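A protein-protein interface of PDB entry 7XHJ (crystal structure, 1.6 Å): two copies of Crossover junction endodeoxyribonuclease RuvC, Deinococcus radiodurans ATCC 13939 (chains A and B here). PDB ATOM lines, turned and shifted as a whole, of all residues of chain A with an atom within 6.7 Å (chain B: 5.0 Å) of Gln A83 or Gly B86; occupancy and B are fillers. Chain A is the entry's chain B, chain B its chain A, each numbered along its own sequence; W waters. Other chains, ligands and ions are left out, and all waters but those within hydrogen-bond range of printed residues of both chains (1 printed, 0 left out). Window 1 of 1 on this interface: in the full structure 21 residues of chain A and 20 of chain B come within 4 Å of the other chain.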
ATOM      1  N   LEU A  10     -35.643   9.483  -3.494  1.00  0.00           N
ATOM      2  CA  LEU A  10     -34.691   9.164  -4.555  1.00  0.00           C
ATOM      3  C   LEU A  10     -35.074   9.855  -5.865  1.00  0.00           C
ATOM      4  O   LEU A  10     -34.253  10.547  -6.481  1.00  0.00           O
ATOM      5  CB  LEU A  10     -34.620   7.643  -4.744  1.00  0.00           C
ATOM      6  CG  LEU A  10     -33.391   6.971  -5.362  1.00  0.00           C
ATOM      7  CD1 LEU A  10     -33.828   5.675  -6.043  1.00  0.00           C
ATOM      8  CD2 LEU A  10     -32.605   7.858  -6.316  1.00  0.00           C
ATOM      9  N   MET A  41     -28.326   3.285  -9.958  1.00  0.00           N
ATOM     10  CA  MET A  41     -28.464   3.760  -8.576  1.00  0.00           C
ATOM     11  C   MET A  41     -27.264   4.553  -8.078  1.00  0.00           C
ATOM     12  O   MET A  41     -27.471   5.609  -7.456  1.00  0.00           O
ATOM     13  CB  MET A  41     -28.749   2.593  -7.616  1.00  0.00           C
ATOM     14  CG  MET A  41     -28.991   3.044  -6.171  1.00  0.00           C
ATOM     15  SD  MET A  41     -30.468   4.086  -6.002  1.00  0.00           S
ATOM     16  CE  MET A  41     -31.706   2.937  -6.565  1.00  0.00           C
ATOM     17  N   PRO A  42     -26.014   4.131  -8.281  1.00  0.00           N
ATOM     18  CA  PRO A  42     -24.903   4.927  -7.742  1.00  0.00           C
ATOM     19  C   PRO A  42     -24.856   6.342  -8.299  1.00  0.00           C
ATOM     20  O   PRO A  42     -24.568   7.286  -7.549  1.00  0.00           O
ATOM     21  CB  PRO A  42     -23.662   4.108  -8.133  1.00  0.00           C
ATOM     22  CG  PRO A  42     -24.178   2.692  -8.231  1.00  0.00           C
ATOM     23  CD  PRO A  42     -25.549   2.840  -8.836  1.00  0.00           C
ATOM     24  N   LEU A  45     -27.555   8.458  -6.597  1.00  0.00           N
ATOM     25  CA  LEU A  45     -27.112   8.841  -5.258  1.00  0.00           C
ATOM     26  C   LEU A  45     -26.023   9.910  -5.297  1.00  0.00           C
ATOM     27  O   LEU A  45     -26.007  10.816  -4.447  1.00  0.00           O
ATOM     28  CB  LEU A  45     -26.615   7.604  -4.507  1.00  0.00           C
ATOM     29  CG  LEU A  45     -27.713   6.562  -4.249  1.00  0.00           C
ATOM     30  CD1 LEU A  45     -27.042   5.317  -3.648  1.00  0.00           C
ATOM     31  CD2 LEU A  45     -28.779   7.116  -3.311  1.00  0.00           C
ATOM     32  N   ASP A  76     -37.688  -4.613   1.147  1.00  0.00           N
ATOM     33  CA  ASP A  76     -36.868  -4.084   0.059  1.00  0.00           C
ATOM     34  C   ASP A  76     -37.255  -2.649  -0.272  1.00  0.00           C
ATOM     35  O   ASP A  76     -36.429  -1.896  -0.800  1.00  0.00           O
ATOM     36  CB  ASP A  76     -36.958  -4.973  -1.181  1.00  0.00           C
ATOM     37  CG  ASP A  76     -35.746  -4.832  -2.100  1.00  0.00           C
ATOM     38  OD1 ASP A  76     -34.859  -3.992  -1.824  1.00  0.00           O
ATOM     39  OD2 ASP A  76     -35.677  -5.576  -3.100  1.00  0.00           O
ATOM     40  N   ALA A  78     -38.132  -0.493   2.267  1.00  0.00           N
ATOM     41  CA  ALA A  78     -37.326   0.124   3.323  1.00  0.00           C
ATOM     42  C   ALA A  78     -35.859   0.211   2.922  1.00  0.00           C
ATOM     43  O   ALA A  78     -35.202   1.233   3.154  1.00  0.00           O
ATOM     44  CB  ALA A  78     -37.467  -0.670   4.624  1.00  0.00           C
ATOM     45  N   PHE A  79     -35.335  -0.851   2.308  1.00  0.00           N
ATOM     46  CA  PHE A  79     -33.932  -0.875   1.901  1.00  0.00           C
ATOM     47  C   PHE A  79     -33.641   0.222   0.879  1.00  0.00           C
ATOM     48  O   PHE A  79     -32.637   0.937   0.983  1.00  0.00           O
ATOM     49  CB  PHE A  79     -33.591  -2.254   1.325  1.00  0.00           C
ATOM     50  CG  PHE A  79     -32.122  -2.462   1.056  1.00  0.00           C
ATOM     51  CD1 PHE A  79     -31.287  -2.913   2.053  1.00  0.00           C
ATOM     52  CD2 PHE A  79     -31.592  -2.246  -0.208  1.00  0.00           C
ATOM     53  CE1 PHE A  79     -29.953  -3.122   1.817  1.00  0.00           C
ATOM     54  CE2 PHE A  79     -30.242  -2.457  -0.455  1.00  0.00           C
ATOM     55  CZ  PHE A  79     -29.423  -2.893   0.566  1.00  0.00           C
ATOM     56  N   LYS A  80     -34.526   0.376  -0.110  1.00  0.00           N
ATOM     57  CA  LYS A  80     -34.328   1.383  -1.146  1.00  0.00           C
ATOM     58  C   LYS A  80     -34.488   2.794  -0.590  1.00  0.00           C
ATOM     59  O   LYS A  80     -33.684   3.685  -0.894  1.00  0.00           O
ATOM     60  CB  LYS A  80     -35.301   1.131  -2.303  1.00  0.00           C
ATOM     61  CG  LYS A  80     -35.269   2.201  -3.387  1.00  0.00           C
ATOM     62  CD  LYS A  80     -36.146   1.799  -4.568  1.00  0.00           C
ATOM     63  CE  LYS A  80     -36.464   2.985  -5.461  1.00  0.00           C
ATOM     64  NZ  LYS A  80     -37.294   3.990  -4.739  1.00  0.00           N
ATOM     65  N   VAL A  81     -35.511   3.020   0.237  1.00  0.00           N
ATOM     66  CA  VAL A  81     -35.652   4.316   0.900  1.00  0.00           C
ATOM     67  C   VAL A  81     -34.409   4.621   1.725  1.00  0.00           C
ATOM     68  O   VAL A  81     -33.929   5.763   1.764  1.00  0.00           O
ATOM     69  CB  VAL A  81     -36.925   4.336   1.764  1.00  0.00           C
ATOM     70  CG1 VAL A  81     -36.944   5.553   2.678  1.00  0.00           C
ATOM     71  CG2 VAL A  81     -38.158   4.312   0.872  1.00  0.00           C
ATOM     72  N   GLY A  82     -33.852   3.593   2.371  1.00  0.00           N
ATOM     73  CA  GLY A  82     -32.652   3.796   3.171  1.00  0.00           C
ATOM     74  C   GLY A  82     -31.450   4.263   2.369  1.00  0.00           C
ATOM     75  O   GLY A  82     -30.653   5.061   2.859  1.00  0.00           O
ATOM     76  N   GLN A  83     -31.288   3.755   1.141  1.00  0.00           N
ATOM     77  CA  GLN A  83     -30.130   4.147   0.332  1.00  0.00           C
ATOM     78  C   GLN A  83     -30.059   5.659   0.157  1.00  0.00           C
ATOM     79  O   GLN A  83     -29.007   6.267   0.371  1.00  0.00           O
ATOM     80  CB  GLN A  83     -30.161   3.451  -1.024  1.00  0.00           C
ATOM     81  CG  GLN A  83     -29.928   1.951  -0.904  1.00  0.00           C
ATOM     82  CD  GLN A  83     -30.294   1.201  -2.181  1.00  0.00           C
ATOM     83  OE1 GLN A  83     -31.356   0.590  -2.272  1.00  0.00           O
ATOM     84  NE2 GLN A  83     -29.420   1.261  -3.171  1.00  0.00           N
ATOM     85  N   ALA A  84     -31.180   6.284  -0.204  1.00  0.00           N
ATOM     86  CA  ALA A  84     -31.195   7.730  -0.366  1.00  0.00           C
ATOM     87  C   ALA A  84     -31.075   8.437   0.979  1.00  0.00           C
ATOM     88  O   ALA A  84     -30.361   9.441   1.109  1.00  0.00           O
ATOM     89  CB  ALA A  84     -32.480   8.159  -1.081  1.00  0.00           C
ATOM     90  N   PHE A  85     -31.752   7.922   2.002  1.00  0.00           N
ATOM     91  CA  PHE A  85     -31.649   8.537   3.319  1.00  0.00           C
ATOM     92  C   PHE A  85     -30.210   8.513   3.819  1.00  0.00           C
ATOM     93  O   PHE A  85     -29.736   9.490   4.408  1.00  0.00           O
ATOM     94  CB  PHE A  85     -32.591   7.809   4.283  1.00  0.00           C
ATOM     95  CG  PHE A  85     -32.981   8.598   5.491  1.00  0.00           C
ATOM     96  CD1 PHE A  85     -34.091   9.434   5.451  1.00  0.00           C
ATOM     97  CD2 PHE A  85     -32.277   8.476   6.676  1.00  0.00           C
ATOM     98  CE1 PHE A  85     -34.479  10.158   6.572  1.00  0.00           C
ATOM     99  CE2 PHE A  85     -32.654   9.194   7.803  1.00  0.00           C
ATOM    100  CZ  PHE A  85     -33.758  10.040   7.750  1.00  0.00           C
ATOM    101  N   GLY A  86     -29.489   7.421   3.559  1.00  0.00           N
ATOM    102  CA  GLY A  86     -28.109   7.329   4.018  1.00  0.00           C
ATOM    103  C   GLY A  86     -27.201   8.396   3.428  1.00  0.00           C
ATOM    104  O   GLY A  86     -26.337   8.946   4.119  1.00  0.00           O
ATOM    105  N   VAL A  87     -27.360   8.686   2.139  1.00  0.00           N
ATOM    106  CA  VAL A  87     -26.508   9.666   1.504  1.00  0.00           C
ATOM    107  C   VAL A  87     -26.840  11.075   1.984  1.00  0.00           C
ATOM    108  O   VAL A  87     -25.947  11.932   2.096  1.00  0.00           O
ATOM    109  CB  VAL A  87     -26.670   9.442  -0.007  1.00  0.00           C
ATOM    110  CG1 VAL A  87     -26.445  10.679  -0.793  1.00  0.00           C
ATOM    111  CG2 VAL A  87     -25.784   8.246  -0.418  1.00  0.00           C
ATOM    112  N   VAL A  88     -28.115  11.324   2.314  1.00  0.00           N
ATOM    113  CA  VAL A  88     -28.505  12.587   2.920  1.00  0.00           C
ATOM    114  C   VAL A  88     -27.890  12.731   4.301  1.00  0.00           C
ATOM    115  O   VAL A  88     -27.328  13.777   4.641  1.00  0.00           O
ATOM    116  CB  VAL A  88     -30.038  12.683   2.982  1.00  0.00           C
ATOM    117  CG1 VAL A  88     -30.467  13.910   3.829  1.00  0.00           C
ATOM    118  CG2 VAL A  88     -30.623  12.726   1.577  1.00  0.00           C
ATOM    119  N   GLY B  82     -29.788  -0.497   4.339  1.00  0.00           N
ATOM    120  CA  GLY B  82     -29.873   0.233   3.083  1.00  0.00           C
ATOM    121  C   GLY B  82     -29.112   1.543   3.125  1.00  0.00           C
ATOM    122  O   GLY B  82     -28.502   1.955   2.131  1.00  0.00           O
ATOM    123  N   GLN B  83     -29.142   2.221   4.273  1.00  0.00           N
ATOM    124  CA  GLN B  83     -28.360   3.445   4.404  1.00  0.00           C
ATOM    125  C   GLN B  83     -26.879   3.168   4.174  1.00  0.00           C
ATOM    126  O   GLN B  83     -26.200   3.925   3.476  1.00  0.00           O
ATOM    127  CB  GLN B  83     -28.567   4.068   5.775  1.00  0.00           C
ATOM    128  CG  GLN B  83     -29.990   4.570   5.983  1.00  0.00           C
ATOM    129  CD  GLN B  83     -30.132   5.365   7.274  1.00  0.00           C
ATOM    130  OE1 GLN B  83     -29.422   6.346   7.492  1.00  0.00           O
ATOM    131  NE2 GLN B  83     -31.043   4.944   8.121  1.00  0.00           N
ATOM    132  N   ALA B  84     -26.360   2.097   4.764  1.00  0.00           N
ATOM    133  CA  ALA B  84     -24.951   1.762   4.557  1.00  0.00           C
ATOM    134  C   ALA B  84     -24.662   1.415   3.101  1.00  0.00           C
ATOM    135  O   ALA B  84     -23.631   1.826   2.548  1.00  0.00           O
ATOM    136  CB  ALA B  84     -24.559   0.613   5.487  1.00  0.00           C
ATOM    137  N   PHE B  85     -25.559   0.661   2.467  1.00  0.00           N
ATOM    138  CA  PHE B  85     -25.402   0.301   1.061  1.00  0.00           C
ATOM    139  C   PHE B  85     -25.376   1.548   0.190  1.00  0.00           C
ATOM    140  O   PHE B  85     -24.583   1.647  -0.753  1.00  0.00           O
ATOM    141  CB  PHE B  85     -26.552  -0.627   0.665  1.00  0.00           C
ATOM    142  CG  PHE B  85     -26.322  -1.427  -0.594  1.00  0.00           C
ATOM    143  CD1 PHE B  85     -25.648  -2.639  -0.548  1.00  0.00           C
ATOM    144  CD2 PHE B  85     -26.848  -1.009  -1.801  1.00  0.00           C
ATOM    145  CE1 PHE B  85     -25.465  -3.401  -1.699  1.00  0.00           C
ATOM    146  CE2 PHE B  85     -26.673  -1.770  -2.969  1.00  0.00           C
ATOM    147  CZ  PHE B  85     -25.974  -2.960  -2.913  1.00  0.00           C
ATOM    148  N   GLY B  86     -26.215   2.532   0.513  1.00  0.00           N
ATOM    149  CA  GLY B  86     -26.211   3.769  -0.254  1.00  0.00           C
ATOM    150  C   GLY B  86     -24.883   4.502  -0.196  1.00  0.00           C
ATOM    151  O   GLY B  86     -24.395   4.998  -1.212  1.00  0.00           O
ATOM    152  N   VAL B  87     -24.287   4.571   0.987  1.00  0.00           N
ATOM    153  CA  VAL B  87     -23.039   5.291   1.152  1.00  0.00           C
ATOM    154  C   VAL B  87     -21.898   4.539   0.474  1.00  0.00           C
ATOM    155  O   VAL B  87     -20.975   5.150  -0.083  1.00  0.00           O
ATOM    156  CB  VAL B  87     -22.806   5.523   2.651  1.00  0.00           C
ATOM    157  CG1 VAL B  87     -21.389   5.809   2.921  1.00  0.00           C
ATOM    158  CG2 VAL B  87     -23.714   6.659   3.147  1.00  0.00           C
ATOM    159  N   VAL B  88     -21.963   3.203   0.482  1.00  0.00           N
ATOM    160  CA  VAL B  88     -20.982   2.388  -0.240  1.00  0.00           C
ATOM    161  C   VAL B  88     -21.072   2.656  -1.734  1.00  0.00           C
ATOM    162  O   VAL B  88     -20.057   2.914  -2.389  1.00  0.00           O
ATOM    163  CB  VAL B  88     -21.178   0.887   0.065  1.00  0.00           C
ATOM    164  CG1 VAL B  88     -20.396   0.022  -0.939  1.00  0.00           C
ATOM    165  CG2 VAL B  88     -20.771   0.572   1.508  1.00  0.00           C
ATOM    166  N   GLN B  89     -22.295   2.614  -2.295  1.00  0.00           N
ATOM    167  CA  GLN B  89     -22.474   2.911  -3.713  1.00  0.00           C
ATOM    168  C   GLN B  89     -21.987   4.312  -4.048  1.00  0.00           C
ATOM    169  O   GLN B  89     -21.394   4.539  -5.108  1.00  0.00           O
ATOM    170  CB  GLN B  89     -23.934   2.756  -4.106  1.00  0.00           C
ATOM    171  CG  GLN B  89     -24.475   1.340  -4.052  1.00  0.00           C
ATOM    172  CD  GLN B  89     -25.975   1.343  -4.284  1.00  0.00           C
ATOM    173  OE1 GLN B  89     -26.742   1.802  -3.447  1.00  0.00           O
ATOM    174  NE2 GLN B  89     -26.390   0.866  -5.437  1.00  0.00           N
ATOM    175  N   LEU B  90     -22.221   5.263  -3.145  1.00  0.00           N
ATOM    176  CA  LEU B  90     -21.792   6.636  -3.367  1.00  0.00           C
ATOM    177  C   LEU B  90     -20.284   6.732  -3.466  1.00  0.00           C
ATOM    178  O   LEU B  90     -19.754   7.405  -4.362  1.00  0.00           O
ATOM    179  CB  LEU B  90     -22.293   7.525  -2.229  1.00  0.00           C
ATOM    180  CG  LEU B  90     -21.775   8.961  -2.284  1.00  0.00           C
ATOM    181  CD1 LEU B  90     -22.365   9.733  -3.482  1.00  0.00           C
ATOM    182  CD2 LEU B  90     -22.122   9.653  -0.974  1.00  0.00           C
HETATM  183  O   HOH W   1     -29.038  -0.423  -5.856  1.00  0.00           O
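The backbone carbonyl oxygen (O) of Gly B82 sits close to the backbone NH (N) of Gln A83 (3.5 Å).
The side-chain amide oxygen (OE1) of Gln B89 sits at hydrogen-bond distance from the side-chain amide nitrogen (NE2) of Gln A83.
The side-chain amide oxygen (OE1) of Gln B89 sits close to the backbone carbonyl oxygen (O) of Phe B85 (3.5 Å).
Water W1 lies within hydrogen-bond range of the side-chain amide nitrogen (NE2) of Gln B89 (3.0 Å) and the side-chain amide nitrogen (NE2) of Gln A83 (3.2 Å).
Hydrophobic or aromatic side chains of chain B within 4 Å of the printed part of chain A: Phe B85, Val B87 and Leu B90.
Along chain B the printed residues that touch a printed residue of chain A span positions 82 to 90.
Of the 16 printed residues of chain A, 9 touch a printed residue of chain B.
Among the printed residues, 18 pairs touch across the chains.
Among the printed residues, no Asp or Glu carboxylate lies within 4 Å of a Lys or Arg side-chain nitrogen of the other chain.
CG of Met A41 touches NE2 of Gln B89, 3.5 Å away.
Gln B89 touches Leu A45 (OE1 to CD1, 3.5 Å).
Leu B90 touches Leu A45 (CD1 to O, 3.9 Å).
CZ of Phe A79 touches CG of Phe B85, 3.6 Å away.
Gly A82 touches Gly B82.
NE2 of Gln A83 touches CD2 of Phe B85, 3.7 Å away.
Gly B86 touches Gln A83.
CD2 of Phe A85 touches OE1 of Gln B83, at 3.7 Å.
Gln B83 touches Gly A86 (CB to CA, 3.7 Å).
Val A87 touches Gly B86 (CG2 to O, 3.6 Å).
Of chain B, only Gly B82, Phe B85, Gly B86 and Gln B89 come within 4 Å of Gln A83.
Gly B86 touches just these residues of chain A: Leu A45, Gln A83 and Val A87.
Printed residues of chain A within 4 Å of Gln B83: Gly A82 (3.2 Å), Phe A85 (3.7 Å) and Gly A86 (3.7 Å).
Printed residues of chain A within 4 Å of Val B87: Gly A86.
Printed residues of chain A within 4 Å of Phe B85: Phe A79 and Gln A83.
Of the printed residues of chain A, Gln B89 touches Met A41, Pro A42, Leu A45 and Gln A83.
Of the printed residues of chain B, Phe A85 touches Gln B83.
The nearest residue of chain B that does not touch Gln A83 is Gln B83 (4.1 Å).
The nearest printed residue of chain A that does not touch Gly B86 is Ala A84 (5.6 Å).
The nearest printed residue of chain A that does not touch Gln B89 is Phe A79 (6.3 Å).
Gly B82 touches its own counterpart, Gly A82.
Gly A82 touches Gln B83, and with the chains exchanged Gln A83 touches Gly B82.
Gln A83 touches Phe B85, and with the chains exchanged Phe A85 touches Gln B83.
Gln A83 touches Gly B86, and with the chains exchanged Gly A86 touches Gln B83.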
